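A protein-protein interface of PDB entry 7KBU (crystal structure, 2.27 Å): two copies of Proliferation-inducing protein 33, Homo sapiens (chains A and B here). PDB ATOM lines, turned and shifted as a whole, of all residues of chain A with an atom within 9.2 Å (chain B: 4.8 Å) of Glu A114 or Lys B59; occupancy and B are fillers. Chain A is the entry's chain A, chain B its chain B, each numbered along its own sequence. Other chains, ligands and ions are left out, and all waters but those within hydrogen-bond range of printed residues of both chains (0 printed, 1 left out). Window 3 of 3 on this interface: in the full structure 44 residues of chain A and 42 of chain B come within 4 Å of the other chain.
Hydrophobic or aromatic side chains of chain B that line the printed part of chain A: Phe B56.
Of the 7 printed residues of chain A, 3 touch a printed residue of chain B.
Among the printed residues, 7 pairs touch across the chains.
Among the printed residues, no Asp or Glu carboxylate lies within 4 Å of a Lys or Arg side-chain nitrogen of the other chain.
No position is printed for both chains.
Of the 7 pairs that touch across the chains among the printed residues, none has its exchanged pair printed and touching as well.
O of Asn A112 lies within hydrogen-bond range of NE of Arg B10 (3.1 Å).
NE2 of Gln B72 is in hydrogen-bond range of OE1 of Glu A114 (2.9 Å).
O of Leu B71 sits at hydrogen-bond distance from NZ of Lys B59, 3.1 Å away.
NZ of Lys B59 sits at hydrogen-bond distance from O of Gly B68.
The side-chain amino group (NZ) of Lys B59 lies within hydrogen-bond range of the backbone carbonyl oxygen (O) of His B69 (3.2 Å).
O of Leu A108 lies within hydrogen-bond range of ND2 of Asn A112 (2.9 Å).
Of the printed residues of chain B, Asn A112 touches Arg B10 (3.1 Å) and Phe B56 (3.3 Å).
Of the printed residues of chain B, Ser A113 touches Arg B10 and Phe B56.
Of the printed residues of chain A, Arg B10 touches Asn A112 and Ser A113.
Leu B55 touches none of the printed residues of chain A.
Of the printed residues of chain A, Phe B56 touches Asn A112 (3.3 Å), Ser A113 (3.8 Å) and Glu A114 (3.4 Å).
Of chain A, only Glu A114 comes within 4 Å of Lys B59.
Printed residues of chain A within 4 Å of Gln B72: Glu A114 (2.9 Å).
The nearest residue of chain B that does not touch Glu A114 is Arg B10 (4.4 Å).
Among the printed residues, merely in contact across the chains: Asn A112 with Phe B56 (3.3 Å), Glu A114 with Phe B56 (3.4 Å), Ser A113 with Arg B10 (3.4 Å), Glu A114 with Lys B59 (3.6 Å) and Ser A113 with Phe B56 (3.8 Å).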
ATOM      1  N   LEU A 108      -6.838  -2.781  -2.678  1.00  0.00           N
ATOM      2  CA  LEU A 108      -6.497  -1.718  -3.616  1.00  0.00           C
ATOM      3  C   LEU A 108      -5.943  -0.489  -2.893  1.00  0.00           C
ATOM      4  O   LEU A 108      -5.044   0.187  -3.406  1.00  0.00           O
ATOM      5  CB  LEU A 108      -7.728  -1.357  -4.452  1.00  0.00           C
ATOM      6  CG  LEU A 108      -7.507  -0.392  -5.617  1.00  0.00           C
ATOM      7  CD1 LEU A 108      -6.642  -1.025  -6.712  1.00  0.00           C
ATOM      8  CD2 LEU A 108      -8.845   0.066  -6.181  1.00  0.00           C
ATOM      9  N   TYR A 109      -6.474  -0.174  -1.710  1.00  0.00           N
ATOM     10  CA  TYR A 109      -5.953   0.951  -0.938  1.00  0.00           C
ATOM     11  C   TYR A 109      -4.537   0.674  -0.446  1.00  0.00           C
ATOM     12  O   TYR A 109      -3.669   1.550  -0.506  1.00  0.00           O
ATOM     13  CB  TYR A 109      -6.871   1.259   0.253  1.00  0.00           C
ATOM     14  CG  TYR A 109      -6.324   2.345   1.173  1.00  0.00           C
ATOM     15  CD1 TYR A 109      -5.501   2.031   2.252  1.00  0.00           C
ATOM     16  CD2 TYR A 109      -6.642   3.685   0.961  1.00  0.00           C
ATOM     17  CE1 TYR A 109      -4.993   3.036   3.095  1.00  0.00           C
ATOM     18  CE2 TYR A 109      -6.155   4.692   1.795  1.00  0.00           C
ATOM     19  CZ  TYR A 109      -5.330   4.366   2.853  1.00  0.00           C
ATOM     20  OH  TYR A 109      -4.840   5.371   3.654  1.00  0.00           O
ATOM     21  N   GLU A 110      -4.293  -0.524   0.090  1.00  0.00           N
ATOM     22  CA  GLU A 110      -2.975  -0.804   0.657  1.00  0.00           C
ATOM     23  C   GLU A 110      -1.890  -0.798  -0.419  1.00  0.00           C
ATOM     24  O   GLU A 110      -0.783  -0.321  -0.171  1.00  0.00           O
ATOM     25  CB  GLU A 110      -2.981  -2.143   1.404  1.00  0.00           C
ATOM     26  CG  GLU A 110      -3.274  -2.043   2.929  1.00  0.00           C
ATOM     27  CD  GLU A 110      -2.287  -1.142   3.716  1.00  0.00           C
ATOM     28  OE1 GLU A 110      -1.150  -1.585   4.024  1.00  0.00           O
ATOM     29  OE2 GLU A 110      -2.665   0.004   4.057  1.00  0.00           O
ATOM     30  N   ALA A 111      -2.204  -1.274  -1.631  1.00  0.00           N
ATOM     31  CA  ALA A 111      -1.246  -1.211  -2.736  1.00  0.00           C
ATOM     32  C   ALA A 111      -0.932   0.224  -3.161  1.00  0.00           C
ATOM     33  O   ALA A 111       0.146   0.483  -3.698  1.00  0.00           O
ATOM     34  CB  ALA A 111      -1.767  -1.993  -3.942  1.00  0.00           C
ATOM     35  N   ASN A 112      -1.867   1.153  -2.970  1.00  0.00           N
ATOM     36  CA  ASN A 112      -1.700   2.532  -3.408  1.00  0.00           C
ATOM     37  C   ASN A 112      -1.241   3.476  -2.302  1.00  0.00           C
ATOM     38  O   ASN A 112      -0.924   4.629  -2.597  1.00  0.00           O
ATOM     39  CB  ASN A 112      -3.017   3.063  -4.005  1.00  0.00           C
ATOM     40  CG  ASN A 112      -3.191   2.682  -5.469  1.00  0.00           C
ATOM     41  OD1 ASN A 112      -2.636   3.327  -6.363  1.00  0.00           O
ATOM     42  ND2 ASN A 112      -3.948   1.614  -5.720  1.00  0.00           N
ATOM     43  N   SER A 113      -1.192   3.028  -1.053  1.00  0.00           N
ATOM     44  CA  SER A 113      -0.901   3.897   0.069  1.00  0.00           C
ATOM     45  C   SER A 113       0.577   3.791   0.423  1.00  0.00           C
ATOM     46  O   SER A 113       1.382   3.308  -0.379  1.00  0.00           O
ATOM     47  CB  SER A 113      -1.781   3.524   1.266  1.00  0.00           C
ATOM     48  OG  SER A 113      -1.206   2.438   1.977  1.00  0.00           O
ATOM     49  N   GLU A 114       0.936   4.227   1.630  1.00  0.00           N
ATOM     50  CA  GLU A 114       2.272   4.031   2.183  1.00  0.00           C
ATOM     51  C   GLU A 114       2.447   2.558   2.561  1.00  0.00           C
ATOM     52  O   GLU A 114       3.517   1.973   2.383  1.00  0.00           O
ATOM     53  CB  GLU A 114       2.492   4.929   3.408  1.00  0.00           C
ATOM     54  CG  GLU A 114       2.740   6.407   3.100  1.00  0.00           C
ATOM     55  CD  GLU A 114       3.318   7.184   4.290  1.00  0.00           C
ATOM     56  OE1 GLU A 114       2.704   7.175   5.378  1.00  0.00           O
ATOM     57  OE2 GLU A 114       4.386   7.817   4.143  1.00  0.00           O
ATOM     58  N   ARG B  10       6.988   5.468  -0.230  1.00  0.00           N
ATOM     59  CA  ARG B  10       6.157   5.951  -1.325  1.00  0.00           C
ATOM     60  C   ARG B  10       6.264   7.475  -1.392  1.00  0.00           C
ATOM     61  O   ARG B  10       6.264   8.165  -0.368  1.00  0.00           O
ATOM     62  CB  ARG B  10       4.705   5.502  -1.138  1.00  0.00           C
ATOM     63  CG  ARG B  10       3.773   5.947  -2.255  1.00  0.00           C
ATOM     64  CD  ARG B  10       3.084   4.781  -2.987  1.00  0.00           C
ATOM     65  NE  ARG B  10       1.916   5.250  -3.731  1.00  0.00           N
ATOM     66  CZ  ARG B  10       1.637   4.983  -5.005  1.00  0.00           C
ATOM     67  NH1 ARG B  10       2.417   4.210  -5.743  1.00  0.00           N
ATOM     68  NH2 ARG B  10       0.539   5.498  -5.548  1.00  0.00           N
ATOM     69  N   LEU B  55      -0.222  12.528  -5.163  1.00  0.00           N
ATOM     70  CA  LEU B  55      -0.452  12.840  -3.755  1.00  0.00           C
ATOM     71  C   LEU B  55       0.807  12.596  -2.927  1.00  0.00           C
ATOM     72  O   LEU B  55       1.195  13.436  -2.108  1.00  0.00           O
ATOM     73  CB  LEU B  55      -1.619  12.008  -3.226  1.00  0.00           C
ATOM     74  CG  LEU B  55      -2.035  12.170  -1.761  1.00  0.00           C
ATOM     75  CD1 LEU B  55      -3.435  11.588  -1.551  1.00  0.00           C
ATOM     76  CD2 LEU B  55      -1.029  11.530  -0.766  1.00  0.00           C
ATOM     77  N   PHE B  56       1.453  11.438  -3.108  1.00  0.00           N
ATOM     78  CA  PHE B  56       2.636  11.135  -2.301  1.00  0.00           C
ATOM     79  C   PHE B  56       3.863  11.909  -2.784  1.00  0.00           C
ATOM     80  O   PHE B  56       4.730  12.247  -1.969  1.00  0.00           O
ATOM     81  CB  PHE B  56       2.882   9.615  -2.268  1.00  0.00           C
ATOM     82  CG  PHE B  56       1.894   8.872  -1.379  1.00  0.00           C
ATOM     83  CD1 PHE B  56       1.962   8.980   0.004  1.00  0.00           C
ATOM     84  CD2 PHE B  56       0.877   8.109  -1.929  1.00  0.00           C
ATOM     85  CE1 PHE B  56       1.048   8.338   0.814  1.00  0.00           C
ATOM     86  CE2 PHE B  56      -0.043   7.455  -1.114  1.00  0.00           C
ATOM     87  CZ  PHE B  56       0.044   7.577   0.257  1.00  0.00           C
ATOM     88  N   ALA B  57       3.949  12.235  -4.078  1.00  0.00           N
ATOM     89  CA  ALA B  57       4.988  13.173  -4.511  1.00  0.00           C
ATOM     90  C   ALA B  57       4.790  14.529  -3.842  1.00  0.00           C
ATOM     91  O   ALA B  57       5.749  15.138  -3.365  1.00  0.00           O
ATOM     92  CB  ALA B  57       4.994  13.330  -6.036  1.00  0.00           C
ATOM     93  N   THR B  58       3.538  14.998  -3.765  1.00  0.00           N
ATOM     94  CA  THR B  58       3.263  16.254  -3.076  1.00  0.00           C
ATOM     95  C   THR B  58       3.641  16.150  -1.606  1.00  0.00           C
ATOM     96  O   THR B  58       4.271  17.053  -1.042  1.00  0.00           O
ATOM     97  CB  THR B  58       1.793  16.634  -3.229  1.00  0.00           C
ATOM     98  OG1 THR B  58       1.518  16.950  -4.599  1.00  0.00           O
ATOM     99  CG2 THR B  58       1.462  17.846  -2.352  1.00  0.00           C
ATOM    100  N   LYS B  59       3.252  15.048  -0.971  1.00  0.00           N
ATOM    101  CA  LYS B  59       3.606  14.807   0.422  1.00  0.00           C
ATOM    102  C   LYS B  59       5.105  14.942   0.630  1.00  0.00           C
ATOM    103  O   LYS B  59       5.555  15.571   1.596  1.00  0.00           O
ATOM    104  CB  LYS B  59       3.126  13.405   0.836  1.00  0.00           C
ATOM    105  CG  LYS B  59       3.112  13.150   2.335  1.00  0.00           C
ATOM    106  CD  LYS B  59       2.724  11.712   2.668  1.00  0.00           C
ATOM    107  CE  LYS B  59       3.267  11.288   4.043  1.00  0.00           C
ATOM    108  NZ  LYS B  59       2.688  12.064   5.190  1.00  0.00           N
ATOM    109  N   CYS B  60       5.897  14.385  -0.287  1.00  0.00           N
ATOM    110  CA  CYS B  60       7.344  14.461  -0.142  1.00  0.00           C
ATOM    111  C   CYS B  60       7.840  15.907  -0.173  1.00  0.00           C
ATOM    112  O   CYS B  60       8.620  16.320   0.697  1.00  0.00           O
ATOM    113  CB  CYS B  60       8.027  13.627  -1.230  1.00  0.00           C
ATOM    114  SG  CYS B  60       9.797  13.325  -0.885  1.00  0.00           S
ATOM    115  N   ARG B  61       7.411  16.693  -1.173  1.00  0.00           N
ATOM    116  CA  ARG B  61       7.835  18.095  -1.245  1.00  0.00           C
ATOM    117  C   ARG B  61       7.499  18.861   0.034  1.00  0.00           C
ATOM    118  O   ARG B  61       8.152  19.866   0.335  1.00  0.00           O
ATOM    119  CB  ARG B  61       7.206  18.788  -2.460  1.00  0.00           C
ATOM    120  N   LEU B  62       6.513  18.395   0.798  1.00  0.00           N
ATOM    121  CA  LEU B  62       6.052  19.057   2.009  1.00  0.00           C
ATOM    122  C   LEU B  62       6.562  18.398   3.287  1.00  0.00           C
ATOM    123  O   LEU B  62       6.076  18.730   4.375  1.00  0.00           O
ATOM    124  CB  LEU B  62       4.518  19.081   2.031  1.00  0.00           C
ATOM    125  CG  LEU B  62       3.818  19.849   0.904  1.00  0.00           C
ATOM    126  CD1 LEU B  62       2.335  19.834   1.134  1.00  0.00           C
ATOM    127  CD2 LEU B  62       4.326  21.280   0.797  1.00  0.00           C
ATOM    128  N   GLU B  63       7.513  17.468   3.191  1.00  0.00           N
ATOM    129  CA  GLU B  63       8.001  16.785   4.387  1.00  0.00           C
ATOM    130  C   GLU B  63       8.609  17.781   5.373  1.00  0.00           C
ATOM    131  O   GLU B  63       9.279  18.744   4.984  1.00  0.00           O
ATOM    132  CB  GLU B  63       9.027  15.704   4.030  1.00  0.00           C
ATOM    133  CG  GLU B  63       9.595  14.988   5.262  1.00  0.00           C
ATOM    134  CD  GLU B  63       9.903  13.511   5.033  1.00  0.00           C
ATOM    135  OE1 GLU B  63      10.096  13.105   3.866  1.00  0.00           O
ATOM    136  OE2 GLU B  63       9.964  12.753   6.028  1.00  0.00           O
ATOM    137  N   GLY B  68       2.385  18.586   5.681  1.00  0.00           N
ATOM    138  CA  GLY B  68       3.086  17.453   5.098  1.00  0.00           C
ATOM    139  C   GLY B  68       2.883  16.160   5.867  1.00  0.00           C
ATOM    140  O   GLY B  68       2.570  15.121   5.282  1.00  0.00           O
ATOM    141  N   HIS B  69       3.081  16.197   7.186  1.00  0.00           N
ATOM    142  CA  HIS B  69       3.003  14.969   7.972  1.00  0.00           C
ATOM    143  C   HIS B  69       1.598  14.378   7.974  1.00  0.00           C
ATOM    144  O   HIS B  69       1.441  13.151   7.986  1.00  0.00           O
ATOM    145  CB  HIS B  69       3.474  15.238   9.403  1.00  0.00           C
ATOM    146  CG  HIS B  69       4.959  15.418   9.528  1.00  0.00           C
ATOM    147  ND1 HIS B  69       5.608  15.438  10.745  1.00  0.00           N
ATOM    148  CD2 HIS B  69       5.920  15.586   8.588  1.00  0.00           C
ATOM    149  CE1 HIS B  69       6.902  15.611  10.548  1.00  0.00           C
ATOM    150  NE2 HIS B  69       7.120  15.703   9.250  1.00  0.00           N
ATOM    151  N   GLN B  70       0.571  15.226   7.933  1.00  0.00           N
ATOM    152  CA  GLN B  70      -0.803  14.741   8.034  1.00  0.00           C
ATOM    153  C   GLN B  70      -1.249  14.018   6.764  1.00  0.00           C
ATOM    154  O   GLN B  70      -1.938  12.992   6.838  1.00  0.00           O
ATOM    155  CB  GLN B  70      -1.732  15.920   8.338  1.00  0.00           C
ATOM    156  CG  GLN B  70      -3.104  15.523   8.881  1.00  0.00           C
ATOM    157  CD  GLN B  70      -4.140  15.219   7.787  1.00  0.00           C
ATOM    158  OE1 GLN B  70      -3.843  15.248   6.587  1.00  0.00           O
ATOM    159  NE2 GLN B  70      -5.368  14.936   8.210  1.00  0.00           N
ATOM    160  N   LEU B  71      -0.837  14.515   5.600  1.00  0.00           N
ATOM    161  CA  LEU B  71      -1.413  14.107   4.326  1.00  0.00           C
ATOM    162  C   LEU B  71      -1.258  12.604   4.084  1.00  0.00           C
ATOM    163  O   LEU B  71      -0.148  12.076   4.039  1.00  0.00           O
ATOM    164  CB  LEU B  71      -0.745  14.904   3.202  1.00  0.00           C
ATOM    165  CG  LEU B  71      -1.185  14.627   1.764  1.00  0.00           C
ATOM    166  CD1 LEU B  71      -2.671  14.950   1.582  1.00  0.00           C
ATOM    167  CD2 LEU B  71      -0.316  15.420   0.770  1.00  0.00           C
ATOM    168  N   GLN B  72      -2.390  11.930   3.896  1.00  0.00           N
ATOM    169  CA  GLN B  72      -2.453  10.525   3.548  1.00  0.00           C
ATOM    170  C   GLN B  72      -3.497  10.337   2.455  1.00  0.00           C
ATOM    171  O   GLN B  72      -4.289  11.236   2.166  1.00  0.00           O
ATOM    172  CB  GLN B  72      -2.816   9.666   4.767  1.00  0.00           C
ATOM    173  CG  GLN B  72      -1.728   9.643   5.835  1.00  0.00           C
ATOM    174  CD  GLN B  72      -0.580   8.717   5.478  1.00  0.00           C
ATOM    175  OE1 GLN B  72      -0.683   7.904   4.561  1.00  0.00           O
ATOM    176  NE2 GLN B  72       0.523   8.840   6.204  1.00  0.00           N
